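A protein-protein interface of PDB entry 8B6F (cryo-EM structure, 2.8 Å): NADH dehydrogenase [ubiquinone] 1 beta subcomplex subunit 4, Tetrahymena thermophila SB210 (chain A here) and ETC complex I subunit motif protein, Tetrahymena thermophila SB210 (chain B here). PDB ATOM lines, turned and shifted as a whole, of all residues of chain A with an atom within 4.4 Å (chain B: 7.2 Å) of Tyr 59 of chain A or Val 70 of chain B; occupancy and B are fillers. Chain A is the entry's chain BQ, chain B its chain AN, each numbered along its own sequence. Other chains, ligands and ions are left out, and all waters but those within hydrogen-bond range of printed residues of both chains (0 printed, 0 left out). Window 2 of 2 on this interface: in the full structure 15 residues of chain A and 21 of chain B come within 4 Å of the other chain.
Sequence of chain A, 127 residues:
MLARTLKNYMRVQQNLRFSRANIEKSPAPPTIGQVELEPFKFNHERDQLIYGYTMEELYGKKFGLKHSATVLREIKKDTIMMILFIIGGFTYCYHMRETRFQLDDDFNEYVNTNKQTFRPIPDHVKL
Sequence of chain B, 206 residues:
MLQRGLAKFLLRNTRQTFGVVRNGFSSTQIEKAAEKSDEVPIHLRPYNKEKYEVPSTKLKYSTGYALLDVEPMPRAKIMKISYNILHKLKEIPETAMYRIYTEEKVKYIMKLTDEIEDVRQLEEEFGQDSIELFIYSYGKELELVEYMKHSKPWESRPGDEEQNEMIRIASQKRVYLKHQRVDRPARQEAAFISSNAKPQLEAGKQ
Printed residues of chain A that touch a printed residue of chain B: Arg 46, Leu 58, Tyr 59 and Lys 62. Of the 16 printed residues of chain B, 6 touch a printed residue of chain A. Along chain B the printed residues that touch a printed residue of chain A span positions 56 to 72. Among the printed residues, Asp or Glu carboxylates within 4 Å of a Lys or Arg side-chain nitrogen of the other chain: Arg 46 of chain A with Asp 69 of chain B (2.9 Å).
Printed residues of chain B within 4 Å of Arg 46 of chain A: Asp 69 (2.9 Å). Glu 57 of chain A touches none of the printed residues of chain B. Of chain B, only Val 70 (3.1 Å) and Pro 72 (3.6 Å) come within 4 Å of Tyr 59 of chain A. Printed residues of chain B within 4 Å of Lys 62 of chain A: Tyr 61. Printed residues of chain A within 4 Å of Ser 56 of chain B: Leu 58 (3.7 Å). Printed residues of chain A within 4 Å of Asp 69 of chain B: Arg 46. Of chain A, only Tyr 59 (3.1 Å) comes within 4 Å of Val 70 of chain B. Of the printed residues of chain A, Pro 72 of chain B touches Tyr 59. Glu 132 of chain B touches none of the printed residues of chain A. The nearest residue of chain B that does not touch Tyr 59 of chain A is Leu 59 of chain B (4.8 Å). The nearest printed residue of chain A that does not touch Asp 69 of chain B is Tyr 59 of chain A (5.8 Å).
NH2 of Arg 46 of chain A is in salt-bridge range of OD2 of Asp 69 of chain B.
O of Ser 56 of chain B touches O of Leu 58 of chain A, at 3.7 Å. Leu 59 of chain B touches Leu 58 of chain A (CD1 to O, 3.5 Å). CE2 of Tyr 59 of chain A touches O of Val 70 of chain B, 3.1 Å away. OH of Tyr 59 of chain A touches CG of Pro 72 of chain B (3.6 Å). Tyr 61 of chain B touches Lys 62 of chain A.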
ATOM      1  N   ARG A  46     -18.967  -1.892  27.489  1.00  0.00           N
ATOM      2  CA  ARG A  46     -20.014  -2.654  28.162  1.00  0.00           C
ATOM      3  C   ARG A  46     -21.022  -1.737  28.840  1.00  0.00           C
ATOM      4  O   ARG A  46     -22.223  -2.025  28.848  1.00  0.00           O
ATOM      5  CB  ARG A  46     -19.401  -3.597  29.194  1.00  0.00           C
ATOM      6  CG  ARG A  46     -18.772  -4.843  28.614  1.00  0.00           C
ATOM      7  CD  ARG A  46     -18.165  -5.694  29.716  1.00  0.00           C
ATOM      8  NE  ARG A  46     -17.651  -6.959  29.211  1.00  0.00           N
ATOM      9  CZ  ARG A  46     -17.042  -7.869  29.958  1.00  0.00           C
ATOM     10  NH1 ARG A  46     -16.846  -7.682  31.252  1.00  0.00           N
ATOM     11  NH2 ARG A  46     -16.618  -8.996  29.393  1.00  0.00           N
ATOM     12  N   ILE A  50     -25.123  -2.081  28.606  1.00  0.00           N
ATOM     13  CA  ILE A  50     -25.851  -2.584  29.765  1.00  0.00           C
ATOM     14  C   ILE A  50     -26.511  -1.436  30.515  1.00  0.00           C
ATOM     15  O   ILE A  50     -27.029  -1.627  31.620  1.00  0.00           O
ATOM     16  CB  ILE A  50     -24.931  -3.382  30.708  1.00  0.00           C
ATOM     17  CG1 ILE A  50     -23.994  -2.434  31.469  1.00  0.00           C
ATOM     18  CG2 ILE A  50     -24.154  -4.430  29.916  1.00  0.00           C
ATOM     19  CD1 ILE A  50     -22.935  -3.125  32.307  1.00  0.00           C
ATOM     20  N   MET A  55     -24.577  -5.992  35.638  1.00  0.00           N
ATOM     21  CA  MET A  55     -23.809  -7.106  35.091  1.00  0.00           C
ATOM     22  C   MET A  55     -24.367  -8.441  35.564  1.00  0.00           C
ATOM     23  O   MET A  55     -24.476  -9.389  34.778  1.00  0.00           O
ATOM     24  CB  MET A  55     -22.338  -6.977  35.485  1.00  0.00           C
ATOM     25  CG  MET A  55     -21.606  -5.834  34.802  1.00  0.00           C
ATOM     26  SD  MET A  55     -21.466  -6.035  33.013  1.00  0.00           S
ATOM     27  CE  MET A  55     -20.448  -7.503  32.900  1.00  0.00           C
ATOM     28  N   GLU A  56     -24.719  -8.541  36.846  1.00  0.00           N
ATOM     29  CA  GLU A  56     -25.341  -9.764  37.342  1.00  0.00           C
ATOM     30  C   GLU A  56     -26.683 -10.011  36.665  1.00  0.00           C
ATOM     31  O   GLU A  56     -27.017 -11.151  36.328  1.00  0.00           O
ATOM     32  CB  GLU A  56     -25.516  -9.693  38.858  1.00  0.00           C
ATOM     33  CG  GLU A  56     -24.218  -9.800  39.634  1.00  0.00           C
ATOM     34  CD  GLU A  56     -24.446  -9.880  41.129  1.00  0.00           C
ATOM     35  OE1 GLU A  56     -25.612  -9.760  41.558  1.00  0.00           O
ATOM     36  OE2 GLU A  56     -23.462 -10.066  41.875  1.00  0.00           O
ATOM     37  N   GLU A  57     -27.472  -8.953  36.465  1.00  0.00           N
ATOM     38  CA  GLU A  57     -28.786  -9.124  35.854  1.00  0.00           C
ATOM     39  C   GLU A  57     -28.673  -9.656  34.430  1.00  0.00           C
ATOM     40  O   GLU A  57     -29.451 -10.525  34.023  1.00  0.00           O
ATOM     41  CB  GLU A  57     -29.545  -7.799  35.868  1.00  0.00           C
ATOM     42  CG  GLU A  57     -29.988  -7.359  37.251  1.00  0.00           C
ATOM     43  CD  GLU A  57     -30.732  -6.040  37.232  1.00  0.00           C
ATOM     44  OE1 GLU A  57     -30.908  -5.472  36.136  1.00  0.00           O
ATOM     45  OE2 GLU A  57     -31.142  -5.571  38.315  1.00  0.00           O
ATOM     46  N   LEU A  58     -27.715  -9.148  33.657  1.00  0.00           N
ATOM     47  CA  LEU A  58     -27.607  -9.514  32.248  1.00  0.00           C
ATOM     48  C   LEU A  58     -26.782 -10.783  32.050  1.00  0.00           C
ATOM     49  O   LEU A  58     -27.279 -11.774  31.506  1.00  0.00           O
ATOM     50  CB  LEU A  58     -26.999  -8.355  31.452  1.00  0.00           C
ATOM     51  CG  LEU A  58     -27.822  -7.067  31.389  1.00  0.00           C
ATOM     52  CD1 LEU A  58     -27.100  -6.043  30.545  1.00  0.00           C
ATOM     53  CD2 LEU A  58     -29.217  -7.316  30.839  1.00  0.00           C
ATOM     54  N   TYR A  59     -25.522 -10.766  32.483  1.00  0.00           N
ATOM     55  CA  TYR A  59     -24.633 -11.900  32.272  1.00  0.00           C
ATOM     56  C   TYR A  59     -24.770 -12.978  33.337  1.00  0.00           C
ATOM     57  O   TYR A  59     -24.215 -14.069  33.162  1.00  0.00           O
ATOM     58  CB  TYR A  59     -23.179 -11.425  32.227  1.00  0.00           C
ATOM     59  CG  TYR A  59     -22.897 -10.407  31.149  1.00  0.00           C
ATOM     60  CD1 TYR A  59     -23.090  -9.052  31.378  1.00  0.00           C
ATOM     61  CD2 TYR A  59     -22.425 -10.801  29.905  1.00  0.00           C
ATOM     62  CE1 TYR A  59     -22.828  -8.118  30.395  1.00  0.00           C
ATOM     63  CE2 TYR A  59     -22.161  -9.876  28.916  1.00  0.00           C
ATOM     64  CZ  TYR A  59     -22.363  -8.536  29.167  1.00  0.00           C
ATOM     65  OH  TYR A  59     -22.100  -7.613  28.183  1.00  0.00           O
ATOM     66  N   GLY A  60     -25.482 -12.710  34.423  1.00  0.00           N
ATOM     67  CA  GLY A  60     -25.567 -13.642  35.525  1.00  0.00           C
ATOM     68  C   GLY A  60     -24.382 -13.514  36.464  1.00  0.00           C
ATOM     69  O   GLY A  60     -23.376 -12.866  36.176  1.00  0.00           O
ATOM     70  N   LYS A  62     -21.064 -14.364  38.461  1.00  0.00           N
ATOM     71  CA  LYS A  62     -19.802 -15.015  38.124  1.00  0.00           C
ATOM     72  C   LYS A  62     -19.087 -15.391  39.413  1.00  0.00           C
ATOM     73  O   LYS A  62     -18.838 -14.529  40.262  1.00  0.00           O
ATOM     74  CB  LYS A  62     -18.919 -14.102  37.274  1.00  0.00           C
ATOM     75  CG  LYS A  62     -19.544 -13.682  35.956  1.00  0.00           C
ATOM     76  CD  LYS A  62     -18.600 -12.789  35.165  1.00  0.00           C
ATOM     77  CE  LYS A  62     -19.208 -12.371  33.837  1.00  0.00           C
ATOM     78  NZ  LYS A  62     -20.477 -11.612  34.016  1.00  0.00           N
ATOM     79  N   SER B  56     -32.003 -11.983  29.616  1.00  0.00           N
ATOM     80  CA  SER B  56     -32.172 -13.403  29.352  1.00  0.00           C
ATOM     81  C   SER B  56     -31.348 -14.203  30.347  1.00  0.00           C
ATOM     82  O   SER B  56     -30.165 -13.913  30.555  1.00  0.00           O
ATOM     83  CB  SER B  56     -31.750 -13.750  27.921  1.00  0.00           C
ATOM     84  OG  SER B  56     -31.816 -15.147  27.694  1.00  0.00           O
ATOM     85  N   LEU B  59     -28.058 -18.266  30.139  1.00  0.00           N
ATOM     86  CA  LEU B  59     -27.016 -17.992  29.165  1.00  0.00           C
ATOM     87  C   LEU B  59     -25.786 -18.849  29.443  1.00  0.00           C
ATOM     88  O   LEU B  59     -25.575 -19.340  30.553  1.00  0.00           O
ATOM     89  CB  LEU B  59     -26.629 -16.511  29.189  1.00  0.00           C
ATOM     90  CG  LEU B  59     -27.669 -15.508  28.683  1.00  0.00           C
ATOM     91  CD1 LEU B  59     -27.162 -14.090  28.877  1.00  0.00           C
ATOM     92  CD2 LEU B  59     -28.012 -15.754  27.221  1.00  0.00           C
ATOM     93  N   LYS B  60     -24.969 -19.023  28.409  1.00  0.00           N
ATOM     94  CA  LYS B  60     -23.730 -19.771  28.556  1.00  0.00           C
ATOM     95  C   LYS B  60     -22.767 -19.023  29.469  1.00  0.00           C
ATOM     96  O   LYS B  60     -22.712 -17.791  29.466  1.00  0.00           O
ATOM     97  CB  LYS B  60     -23.078 -20.006  27.196  1.00  0.00           C
ATOM     98  CG  LYS B  60     -23.878 -20.904  26.268  1.00  0.00           C
ATOM     99  CD  LYS B  60     -23.085 -21.272  25.022  1.00  0.00           C
ATOM    100  CE  LYS B  60     -22.709 -20.052  24.197  1.00  0.00           C
ATOM    101  NZ  LYS B  60     -23.895 -19.244  23.805  1.00  0.00           N
ATOM    102  N   TYR B  61     -22.007 -19.780  30.260  1.00  0.00           N
ATOM    103  CA  TYR B  61     -21.003 -19.164  31.118  1.00  0.00           C
ATOM    104  C   TYR B  61     -19.839 -18.616  30.305  1.00  0.00           C
ATOM    105  O   TYR B  61     -19.225 -17.617  30.696  1.00  0.00           O
ATOM    106  CB  TYR B  61     -20.507 -20.180  32.143  1.00  0.00           C
ATOM    107  CG  TYR B  61     -19.839 -19.566  33.347  1.00  0.00           C
ATOM    108  CD1 TYR B  61     -20.566 -18.816  34.262  1.00  0.00           C
ATOM    109  CD2 TYR B  61     -18.487 -19.757  33.585  1.00  0.00           C
ATOM    110  CE1 TYR B  61     -19.962 -18.262  35.370  1.00  0.00           C
ATOM    111  CE2 TYR B  61     -17.873 -19.207  34.689  1.00  0.00           C
ATOM    112  CZ  TYR B  61     -18.616 -18.461  35.578  1.00  0.00           C
ATOM    113  OH  TYR B  61     -18.007 -17.913  36.681  1.00  0.00           O
ATOM    114  N   SER B  62     -19.521 -19.252  29.180  1.00  0.00           N
ATOM    115  CA  SER B  62     -18.472 -18.778  28.293  1.00  0.00           C
ATOM    116  C   SER B  62     -18.798 -19.223  26.876  1.00  0.00           C
ATOM    117  O   SER B  62     -19.533 -20.190  26.662  1.00  0.00           O
ATOM    118  CB  SER B  62     -17.096 -19.296  28.717  1.00  0.00           C
ATOM    119  OG  SER B  62     -17.053 -20.712  28.682  1.00  0.00           O
ATOM    120  N   THR B  63     -18.240 -18.502  25.904  1.00  0.00           N
ATOM    121  CA  THR B  63     -18.479 -18.820  24.501  1.00  0.00           C
ATOM    122  C   THR B  63     -17.649 -19.997  24.011  1.00  0.00           C
ATOM    123  O   THR B  63     -18.027 -20.631  23.021  1.00  0.00           O
ATOM    124  CB  THR B  63     -18.183 -17.602  23.623  1.00  0.00           C
ATOM    125  OG1 THR B  63     -16.857 -17.129  23.886  1.00  0.00           O
ATOM    126  CG2 THR B  63     -19.174 -16.487  23.895  1.00  0.00           C
ATOM    127  N   GLY B  64     -16.537 -20.305  24.675  1.00  0.00           N
ATOM    128  CA  GLY B  64     -15.638 -21.345  24.231  1.00  0.00           C
ATOM    129  C   GLY B  64     -14.514 -20.868  23.338  1.00  0.00           C
ATOM    130  O   GLY B  64     -13.587 -21.641  23.072  1.00  0.00           O
ATOM    131  N   LEU B  68     -13.908 -13.737  22.991  1.00  0.00           N
ATOM    132  CA  LEU B  68     -15.249 -13.697  22.407  1.00  0.00           C
ATOM    133  C   LEU B  68     -16.242 -13.668  23.566  1.00  0.00           C
ATOM    134  O   LEU B  68     -16.670 -14.716  24.054  1.00  0.00           O
ATOM    135  CB  LEU B  68     -15.485 -14.885  21.480  1.00  0.00           C
ATOM    136  CG  LEU B  68     -16.798 -14.888  20.693  1.00  0.00           C
ATOM    137  CD1 LEU B  68     -16.856 -13.724  19.721  1.00  0.00           C
ATOM    138  CD2 LEU B  68     -16.981 -16.203  19.957  1.00  0.00           C
ATOM    139  N   ASP B  69     -16.606 -12.464  24.001  1.00  0.00           N
ATOM    140  CA  ASP B  69     -17.491 -12.307  25.143  1.00  0.00           C
ATOM    141  C   ASP B  69     -18.903 -12.780  24.808  1.00  0.00           C
ATOM    142  O   ASP B  69     -19.295 -12.885  23.644  1.00  0.00           O
ATOM    143  CB  ASP B  69     -17.530 -10.849  25.599  1.00  0.00           C
ATOM    144  CG  ASP B  69     -16.202 -10.376  26.154  1.00  0.00           C
ATOM    145  OD1 ASP B  69     -15.245 -11.179  26.180  1.00  0.00           O
ATOM    146  OD2 ASP B  69     -16.114  -9.202  26.570  1.00  0.00           O
ATOM    147  N   VAL B  70     -19.670 -13.059  25.857  1.00  0.00           N
ATOM    148  CA  VAL B  70     -21.028 -13.573  25.708  1.00  0.00           C
ATOM    149  C   VAL B  70     -21.979 -12.410  25.463  1.00  0.00           C
ATOM    150  O   VAL B  70     -21.969 -11.416  26.198  1.00  0.00           O
ATOM    151  CB  VAL B  70     -21.443 -14.375  26.953  1.00  0.00           C
ATOM    152  CG1 VAL B  70     -22.890 -14.837  26.840  1.00  0.00           C
ATOM    153  CG2 VAL B  70     -20.531 -15.567  27.149  1.00  0.00           C
ATOM    154  N   GLU B  71     -22.796 -12.530  24.423  1.00  0.00           N
ATOM    155  CA  GLU B  71     -23.791 -11.510  24.118  1.00  0.00           C
ATOM    156  C   GLU B  71     -24.970 -11.640  25.080  1.00  0.00           C
ATOM    157  O   GLU B  71     -25.465 -12.751  25.289  1.00  0.00           O
ATOM    158  CB  GLU B  71     -24.270 -11.652  22.676  1.00  0.00           C
ATOM    159  CG  GLU B  71     -25.318 -10.634  22.262  1.00  0.00           C
ATOM    160  CD  GLU B  71     -24.822  -9.208  22.372  1.00  0.00           C
ATOM    161  OE1 GLU B  71     -23.590  -9.006  22.403  1.00  0.00           O
ATOM    162  OE2 GLU B  71     -25.663  -8.287  22.435  1.00  0.00           O
ATOM    163  N   PRO B  72     -25.446 -10.539  25.687  1.00  0.00           N
ATOM    164  CA  PRO B  72     -26.586 -10.654  26.608  1.00  0.00           C
ATOM    165  C   PRO B  72     -27.934 -10.586  25.912  1.00  0.00           C
ATOM    166  O   PRO B  72     -28.941 -11.046  26.460  1.00  0.00           O
ATOM    167  CB  PRO B  72     -26.395  -9.463  27.558  1.00  0.00           C
ATOM    168  CG  PRO B  72     -25.292  -8.617  26.962  1.00  0.00           C
ATOM    169  CD  PRO B  72     -24.977  -9.147  25.605  1.00  0.00           C
ATOM    170  N   MET B  73     -27.972 -10.011  24.711  1.00  0.00           N
ATOM    171  CA  MET B  73     -29.203  -9.856  23.934  1.00  0.00           C
ATOM    172  C   MET B  73     -28.951 -10.304  22.502  1.00  0.00           C
ATOM    173  O   MET B  73     -28.943  -9.491  21.571  1.00  0.00           O
ATOM    174  CB  MET B  73     -29.701  -8.411  23.984  1.00  0.00           C
ATOM    175  CG  MET B  73     -30.003  -7.931  25.395  1.00  0.00           C
ATOM    176  SD  MET B  73     -30.530  -6.212  25.472  1.00  0.00           S
ATOM    177  CE  MET B  73     -30.823  -6.040  27.229  1.00  0.00           C
ATOM    178  N   PRO B  74     -28.734 -11.605  22.288  1.00  0.00           N
ATOM    179  CA  PRO B  74     -28.523 -12.082  20.912  1.00  0.00           C
ATOM    180  C   PRO B  74     -29.684 -11.771  19.987  1.00  0.00           C
ATOM    181  O   PRO B  74     -29.467 -11.414  18.825  1.00  0.00           O
ATOM    182  CB  PRO B  74     -28.327 -13.595  21.091  1.00  0.00           C
ATOM    183  CG  PRO B  74     -27.962 -13.777  22.519  1.00  0.00           C
ATOM    184  CD  PRO B  74     -28.674 -12.702  23.267  1.00  0.00           C
ATOM    185  N   ILE B 131     -23.839 -18.657  19.867  1.00  0.00           N
ATOM    186  CA  ILE B 131     -24.589 -17.638  19.142  1.00  0.00           C
ATOM    187  C   ILE B 131     -23.706 -16.433  18.851  1.00  0.00           C
ATOM    188  O   ILE B 131     -23.932 -15.711  17.874  1.00  0.00           O
ATOM    189  CB  ILE B 131     -25.847 -17.238  19.936  1.00  0.00           C
ATOM    190  CG1 ILE B 131     -26.831 -16.475  19.048  1.00  0.00           C
ATOM    191  CG2 ILE B 131     -25.480 -16.397  21.155  1.00  0.00           C
ATOM    192  CD1 ILE B 131     -27.518 -17.337  18.010  1.00  0.00           C
ATOM    193  N   GLU B 132     -22.685 -16.201  19.676  1.00  0.00           N
ATOM    194  CA  GLU B 132     -21.824 -15.041  19.477  1.00  0.00           C
ATOM    195  C   GLU B 132     -21.051 -15.144  18.172  1.00  0.00           C
ATOM    196  O   GLU B 132     -20.872 -14.145  17.469  1.00  0.00           O
ATOM    197  CB  GLU B 132     -20.866 -14.888  20.657  1.00  0.00           C
ATOM    198  CG  GLU B 132     -21.538 -14.445  21.950  1.00  0.00           C
ATOM    199  CD  GLU B 132     -22.434 -15.508  22.551  1.00  0.00           C
ATOM    200  OE1 GLU B 132     -22.327 -16.681  22.139  1.00  0.00           O
ATOM    201  OE2 GLU B 132     -23.244 -15.172  23.438  1.00  0.00           O
